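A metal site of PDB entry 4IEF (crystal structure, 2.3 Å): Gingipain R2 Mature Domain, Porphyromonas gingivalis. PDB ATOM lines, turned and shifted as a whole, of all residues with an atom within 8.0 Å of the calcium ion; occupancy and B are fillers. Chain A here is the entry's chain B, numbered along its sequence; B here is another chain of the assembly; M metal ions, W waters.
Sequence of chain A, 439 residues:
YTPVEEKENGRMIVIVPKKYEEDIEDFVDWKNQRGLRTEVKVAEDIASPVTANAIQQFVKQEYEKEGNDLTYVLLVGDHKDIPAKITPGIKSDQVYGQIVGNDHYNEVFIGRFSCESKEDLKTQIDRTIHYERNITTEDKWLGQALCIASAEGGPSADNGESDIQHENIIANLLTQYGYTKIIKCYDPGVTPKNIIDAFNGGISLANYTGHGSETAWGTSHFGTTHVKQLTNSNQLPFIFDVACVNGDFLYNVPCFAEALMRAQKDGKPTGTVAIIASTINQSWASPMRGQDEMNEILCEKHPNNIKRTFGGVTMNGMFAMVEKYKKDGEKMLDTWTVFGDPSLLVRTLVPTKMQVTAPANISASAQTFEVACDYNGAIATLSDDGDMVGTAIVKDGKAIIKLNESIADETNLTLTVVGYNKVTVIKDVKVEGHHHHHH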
ATOM      1  N   TYR A  63     -14.294  -5.375  37.520  1.00  0.00           N
ATOM      2  CA  TYR A  63     -13.236  -5.522  36.520  1.00  0.00           C
ATOM      3  C   TYR A  63     -13.363  -4.416  35.459  1.00  0.00           C
ATOM      4  O   TYR A  63     -12.348  -3.849  35.042  1.00  0.00           O
ATOM      5  CB  TYR A  63     -13.328  -6.925  35.874  1.00  0.00           C
ATOM      6  CG  TYR A  63     -12.304  -7.173  34.789  1.00  0.00           C
ATOM      7  CD1 TYR A  63     -11.079  -7.768  35.083  1.00  0.00           C
ATOM      8  CD2 TYR A  63     -12.565  -6.844  33.461  1.00  0.00           C
ATOM      9  CE1 TYR A  63     -10.124  -7.987  34.090  1.00  0.00           C
ATOM     10  CE2 TYR A  63     -11.613  -7.040  32.466  1.00  0.00           C
ATOM     11  CZ  TYR A  63     -10.404  -7.628  32.774  1.00  0.00           C
ATOM     12  OH  TYR A  63      -9.479  -7.856  31.787  1.00  0.00           O
ATOM     13  N   GLY A  97     -12.740 -15.602  38.160  1.00  0.00           N
ATOM     14  CA  GLY A  97     -11.696 -14.830  37.499  1.00  0.00           C
ATOM     15  C   GLY A  97     -11.720 -14.908  35.984  1.00  0.00           C
ATOM     16  O   GLY A  97     -10.938 -14.236  35.314  1.00  0.00           O
ATOM     17  N   GLN A  98     -12.619 -15.763  35.436  1.00  0.00           N
ATOM     18  CA  GLN A  98     -12.822 -15.931  33.997  1.00  0.00           C
ATOM     19  C   GLN A  98     -13.911 -14.936  33.600  1.00  0.00           C
ATOM     20  O   GLN A  98     -15.105 -15.263  33.655  1.00  0.00           O
ATOM     21  CB  GLN A  98     -13.180 -17.393  33.681  1.00  0.00           C
ATOM     22  CG  GLN A  98     -12.019 -18.363  33.883  1.00  0.00           C
ATOM     23  CD  GLN A  98     -12.423 -19.800  34.093  1.00  0.00           C
ATOM     24  OE1 GLN A  98     -13.452 -20.278  33.617  1.00  0.00           O
ATOM     25  NE2 GLN A  98     -11.573 -20.553  34.774  1.00  0.00           N
ATOM     26  N   ILE A  99     -13.503 -13.693  33.263  1.00  0.00           N
ATOM     27  CA  ILE A  99     -14.398 -12.570  33.003  1.00  0.00           C
ATOM     28  C   ILE A  99     -14.492 -12.210  31.520  1.00  0.00           C
ATOM     29  O   ILE A  99     -15.611 -12.026  31.022  1.00  0.00           O
ATOM     30  CB  ILE A  99     -13.944 -11.341  33.854  1.00  0.00           C
ATOM     31  CG1 ILE A  99     -13.994 -11.682  35.360  1.00  0.00           C
ATOM     32  CG2 ILE A  99     -14.755 -10.053  33.550  1.00  0.00           C
ATOM     33  CD1 ILE A  99     -12.867 -11.117  36.146  1.00  0.00           C
ATOM     34  N   VAL A 100     -13.330 -12.073  30.826  1.00  0.00           N
ATOM     35  CA  VAL A 100     -13.318 -11.694  29.406  1.00  0.00           C
ATOM     36  C   VAL A 100     -13.135 -12.941  28.533  1.00  0.00           C
ATOM     37  O   VAL A 100     -12.123 -13.655  28.628  1.00  0.00           O
ATOM     38  CB  VAL A 100     -12.274 -10.600  29.063  1.00  0.00           C
ATOM     39  CG1 VAL A 100     -12.523 -10.038  27.674  1.00  0.00           C
ATOM     40  CG2 VAL A 100     -12.314  -9.473  30.093  1.00  0.00           C
ATOM     41  N   GLY A 101     -14.138 -13.175  27.703  1.00  0.00           N
ATOM     42  CA  GLY A 101     -14.186 -14.285  26.766  1.00  0.00           C
ATOM     43  C   GLY A 101     -14.798 -15.554  27.326  1.00  0.00           C
ATOM     44  O   GLY A 101     -14.703 -15.824  28.513  1.00  0.00           O
ATOM     45  N   ASN A 102     -15.448 -16.335  26.457  1.00  0.00           N
ATOM     46  CA  ASN A 102     -16.028 -17.623  26.810  1.00  0.00           C
ATOM     47  C   ASN A 102     -14.912 -18.673  26.691  1.00  0.00           C
ATOM     48  O   ASN A 102     -14.823 -19.413  25.716  1.00  0.00           O
ATOM     49  CB  ASN A 102     -17.251 -17.941  25.917  1.00  0.00           C
ATOM     50  CG  ASN A 102     -18.036 -19.183  26.304  1.00  0.00           C
ATOM     51  OD1 ASN A 102     -18.139 -19.560  27.485  1.00  0.00           O
ATOM     52  ND2 ASN A 102     -18.646 -19.809  25.321  1.00  0.00           N
ATOM     53  N   ASP A 103     -14.002 -18.639  27.679  1.00  0.00           N
ATOM     54  CA  ASP A 103     -12.810 -19.499  27.791  1.00  0.00           C
ATOM     55  C   ASP A 103     -12.435 -19.659  29.253  1.00  0.00           C
ATOM     56  O   ASP A 103     -13.034 -19.003  30.111  1.00  0.00           O
ATOM     57  CB  ASP A 103     -11.636 -18.911  26.991  1.00  0.00           C
ATOM     58  CG  ASP A 103     -11.357 -17.459  27.298  1.00  0.00           C
ATOM     59  OD1 ASP A 103     -11.744 -16.605  26.477  1.00  0.00           O
ATOM     60  OD2 ASP A 103     -10.780 -17.179  28.389  1.00  0.00           O
ATOM     61  N   HIS A 104     -11.424 -20.500  29.544  1.00  0.00           N
ATOM     62  CA  HIS A 104     -11.007 -20.772  30.917  1.00  0.00           C
ATOM     63  C   HIS A 104      -9.705 -20.045  31.281  1.00  0.00           C
ATOM     64  O   HIS A 104      -9.095 -20.354  32.306  1.00  0.00           O
ATOM     65  CB  HIS A 104     -10.890 -22.295  31.118  1.00  0.00           C
ATOM     66  CG  HIS A 104     -12.180 -23.000  30.866  1.00  0.00           C
ATOM     67  ND1 HIS A 104     -12.992 -23.427  31.903  1.00  0.00           N
ATOM     68  CD2 HIS A 104     -12.815 -23.260  29.695  1.00  0.00           C
ATOM     69  CE1 HIS A 104     -14.050 -23.965  31.330  1.00  0.00           C
ATOM     70  NE2 HIS A 104     -13.992 -23.887  30.007  1.00  0.00           N
ATOM     71  N   TYR A 105      -9.313 -19.052  30.455  1.00  0.00           N
ATOM     72  CA  TYR A 105      -8.132 -18.228  30.719  1.00  0.00           C
ATOM     73  C   TYR A 105      -8.523 -17.076  31.625  1.00  0.00           C
ATOM     74  O   TYR A 105      -9.216 -16.140  31.194  1.00  0.00           O
ATOM     75  CB  TYR A 105      -7.492 -17.722  29.419  1.00  0.00           C
ATOM     76  CG  TYR A 105      -6.690 -18.775  28.684  1.00  0.00           C
ATOM     77  CD1 TYR A 105      -5.295 -18.798  28.771  1.00  0.00           C
ATOM     78  CD2 TYR A 105      -7.313 -19.739  27.896  1.00  0.00           C
ATOM     79  CE1 TYR A 105      -4.550 -19.752  28.066  1.00  0.00           C
ATOM     80  CE2 TYR A 105      -6.580 -20.691  27.198  1.00  0.00           C
ATOM     81  CZ  TYR A 105      -5.190 -20.691  27.282  1.00  0.00           C
ATOM     82  OH  TYR A 105      -4.456 -21.626  26.611  1.00  0.00           O
ATOM     83  N   ASN A 106      -8.127 -17.165  32.895  1.00  0.00           N
ATOM     84  CA  ASN A 106      -8.420 -16.190  33.926  1.00  0.00           C
ATOM     85  C   ASN A 106      -7.780 -14.841  33.668  1.00  0.00           C
ATOM     86  O   ASN A 106      -6.618 -14.752  33.281  1.00  0.00           O
ATOM     87  CB  ASN A 106      -7.970 -16.683  35.296  1.00  0.00           C
ATOM     88  CG  ASN A 106      -8.901 -17.680  35.924  1.00  0.00           C
ATOM     89  OD1 ASN A 106      -9.153 -18.759  35.382  1.00  0.00           O
ATOM     90  ND2 ASN A 106      -9.328 -17.384  37.140  1.00  0.00           N
ATOM     91  N   GLU A 107      -8.564 -13.777  33.918  1.00  0.00           N
ATOM     92  CA  GLU A 107      -8.159 -12.376  33.862  1.00  0.00           C
ATOM     93  C   GLU A 107      -7.713 -11.944  35.254  1.00  0.00           C
ATOM     94  O   GLU A 107      -6.805 -11.139  35.410  1.00  0.00           O
ATOM     95  CB  GLU A 107      -9.358 -11.500  33.412  1.00  0.00           C
ATOM     96  CG  GLU A 107      -9.652 -11.464  31.930  1.00  0.00           C
ATOM     97  CD  GLU A 107      -9.958 -12.781  31.231  1.00  0.00           C
ATOM     98  OE1 GLU A 107      -9.204 -13.097  30.286  1.00  0.00           O
ATOM     99  OE2 GLU A 107     -10.925 -13.481  31.599  1.00  0.00           O
ATOM    100  N   VAL A 108      -8.399 -12.507  36.269  1.00  0.00           N
ATOM    101  CA  VAL A 108      -8.215 -12.220  37.692  1.00  0.00           C
ATOM    102  C   VAL A 108      -7.867 -13.510  38.453  1.00  0.00           C
ATOM    103  O   VAL A 108      -8.436 -14.570  38.178  1.00  0.00           O
ATOM    104  CB  VAL A 108      -9.494 -11.519  38.251  1.00  0.00           C
ATOM    105  CG1 VAL A 108      -9.479 -11.410  39.780  1.00  0.00           C
ATOM    106  CG2 VAL A 108      -9.692 -10.133  37.618  1.00  0.00           C
ATOM    107  N   PHE A 319      -2.090 -22.399  32.658  1.00  0.00           N
ATOM    108  CA  PHE A 319      -2.331 -21.940  31.272  1.00  0.00           C
ATOM    109  C   PHE A 319      -1.729 -22.921  30.266  1.00  0.00           C
ATOM    110  O   PHE A 319      -2.372 -23.226  29.253  1.00  0.00           O
ATOM    111  CB  PHE A 319      -1.782 -20.531  31.043  1.00  0.00           C
ATOM    112  CG  PHE A 319      -2.570 -19.385  31.643  1.00  0.00           C
ATOM    113  CD1 PHE A 319      -3.901 -19.566  32.026  1.00  0.00           C
ATOM    114  CD2 PHE A 319      -2.015 -18.122  31.771  1.00  0.00           C
ATOM    115  CE1 PHE A 319      -4.644 -18.501  32.545  1.00  0.00           C
ATOM    116  CE2 PHE A 319      -2.751 -17.068  32.310  1.00  0.00           C
ATOM    117  CZ  PHE A 319      -4.066 -17.266  32.684  1.00  0.00           C
ATOM    118  N   PHE B 139      -9.466 -18.118  22.478  1.00  0.00           N
ATOM    119  CA  PHE B 139      -9.668 -17.660  23.846  1.00  0.00           C
ATOM    120  C   PHE B 139      -9.268 -16.199  23.984  1.00  0.00           C
ATOM    121  O   PHE B 139      -8.573 -15.664  23.134  1.00  0.00           O
ATOM    122  CB  PHE B 139      -8.843 -18.539  24.823  1.00  0.00           C
ATOM    123  CG  PHE B 139      -7.347 -18.500  24.655  1.00  0.00           C
ATOM    124  CD1 PHE B 139      -6.569 -17.583  25.354  1.00  0.00           C
ATOM    125  CD2 PHE B 139      -6.687 -19.421  23.840  1.00  0.00           C
ATOM    126  CE1 PHE B 139      -5.183 -17.564  25.220  1.00  0.00           C
ATOM    127  CE2 PHE B 139      -5.298 -19.398  23.692  1.00  0.00           C
ATOM    128  CZ  PHE B 139      -4.552 -18.473  24.388  1.00  0.00           C
ATOM    129  N   ILE B 140      -9.700 -15.564  25.083  1.00  0.00           N
ATOM    130  CA  ILE B 140      -9.300 -14.202  25.388  1.00  0.00           C
ATOM    131  C   ILE B 140      -8.566 -14.231  26.728  1.00  0.00           C
ATOM    132  O   ILE B 140      -9.096 -14.724  27.732  1.00  0.00           O
ATOM    133  CB  ILE B 140     -10.461 -13.165  25.353  1.00  0.00           C
ATOM    134  CG1 ILE B 140     -11.099 -13.091  23.923  1.00  0.00           C
ATOM    135  CG2 ILE B 140      -9.965 -11.776  25.809  1.00  0.00           C
ATOM    136  CD1 ILE B 140     -12.537 -12.541  23.861  1.00  0.00           C
ATOM    137  N   LEU B 141      -7.311 -13.748  26.734  1.00  0.00           N
ATOM    138  CA  LEU B 141      -6.489 -13.609  27.921  1.00  0.00           C
ATOM    139  C   LEU B 141      -6.339 -12.113  28.157  1.00  0.00           C
ATOM    140  O   LEU B 141      -5.473 -11.474  27.560  1.00  0.00           O
ATOM    141  CB  LEU B 141      -5.139 -14.347  27.797  1.00  0.00           C
ATOM    142  CG  LEU B 141      -4.147 -14.209  28.971  1.00  0.00           C
ATOM    143  CD1 LEU B 141      -4.767 -14.626  30.298  1.00  0.00           C
ATOM    144  CD2 LEU B 141      -2.869 -14.974  28.692  1.00  0.00           C
ATOM    145  N   ARG B 142      -7.238 -11.562  28.998  1.00  0.00           N
ATOM    146  CA  ARG B 142      -7.354 -10.156  29.376  1.00  0.00           C
ATOM    147  C   ARG B 142      -7.606  -9.270  28.135  1.00  0.00           C
ATOM    148  O   ARG B 142      -8.764  -9.153  27.723  1.00  0.00           O
ATOM    149  CB  ARG B 142      -6.134  -9.689  30.205  1.00  0.00           C
ATOM    150  CG  ARG B 142      -6.401  -8.399  30.962  1.00  0.00           C
ATOM    151  CD  ARG B 142      -5.562  -8.253  32.199  1.00  0.00           C
ATOM    152  NE  ARG B 142      -6.069  -7.165  33.028  1.00  0.00           N
ATOM    153  CZ  ARG B 142      -6.544  -7.311  34.271  1.00  0.00           C
ATOM    154  NH1 ARG B 142      -6.519  -8.498  34.859  1.00  0.00           N
ATOM    155  NH2 ARG B 142      -6.995  -6.261  34.937  1.00  0.00           N
ATOM    156  N   ASP B 143      -6.565  -8.680  27.542  1.00  0.00           N
ATOM    157  CA  ASP B 143      -6.692  -7.783  26.386  1.00  0.00           C
ATOM    158  C   ASP B 143      -6.196  -8.429  25.073  1.00  0.00           C
ATOM    159  O   ASP B 143      -6.187  -7.743  24.041  1.00  0.00           O
ATOM    160  CB  ASP B 143      -5.926  -6.469  26.641  1.00  0.00           C
ATOM    161  CG  ASP B 143      -6.423  -5.680  27.845  1.00  0.00           C
ATOM    162  OD1 ASP B 143      -5.621  -5.442  28.772  1.00  0.00           O
ATOM    163  OD2 ASP B 143      -7.605  -5.299  27.850  1.00  0.00           O
ATOM    164  N   VAL B 144      -5.791  -9.715  25.101  1.00  0.00           N
ATOM    165  CA  VAL B 144      -5.267 -10.381  23.906  1.00  0.00           C
ATOM    166  C   VAL B 144      -6.108 -11.634  23.565  1.00  0.00           C
ATOM    167  O   VAL B 144      -6.353 -12.474  24.437  1.00  0.00           O
ATOM    168  CB  VAL B 144      -3.757 -10.743  24.041  1.00  0.00           C
ATOM    169  CG1 VAL B 144      -3.236 -11.416  22.777  1.00  0.00           C
ATOM    170  CG2 VAL B 144      -2.907  -9.505  24.357  1.00  0.00           C
ATOM    171  N   ASN B 182     -15.717 -16.155  20.061  1.00  0.00           N
ATOM    172  CA  ASN B 182     -15.108 -15.581  21.268  1.00  0.00           C
ATOM    173  C   ASN B 182     -14.200 -14.370  20.918  1.00  0.00           C
ATOM    174  O   ASN B 182     -12.970 -14.432  21.068  1.00  0.00           O
ATOM    175  CB  ASN B 182     -14.321 -16.685  22.012  1.00  0.00           C
ATOM    176  CG  ASN B 182     -14.057 -16.405  23.455  1.00  0.00           C
ATOM    177  OD1 ASN B 182     -14.718 -15.568  24.076  1.00  0.00           O
ATOM    178  ND2 ASN B 182     -13.123 -17.136  24.030  1.00  0.00           N
HETATM  179 CA    CA M   1     -10.622 -15.161  29.677  1.00  0.00          CA
HETATM  180  O   HOH W   1     -12.647 -16.389  30.703  1.00  0.00           O
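The side-chain carboxylate (OD1) of Asp 103 lies within hydrogen-bond range of the side-chain amide nitrogen (ND2) of Asn 182 of chain B, at 2.9 Å. OE2 of Glu 107 lies close to N of Ile 99, 3.1 Å away. The guanidinium group of Arg 142 of chain B lies within hydrogen-bond range of the backbone carbonyl oxygen of Glu 107. N of Glu 107 sits at hydrogen-bond distance from O of Gly 97, at 2.8 Å.
Of the 21 residues printed, 5 come within 4 Å of the calcium ion.
The calcium ion is bound by O of Tyr 105 (2.3 Å), O of Val 100 (2.4 Å), OD2 of Asp 103 (2.4 Å), O of Ile 140 of chain B (2.5 Å), OE2 of Glu 107 (2.6 Å), OE1 of Glu 107 (2.6 Å) and water W1 (2.6 Å). The calcium ion has seven donor atoms within binding distance.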
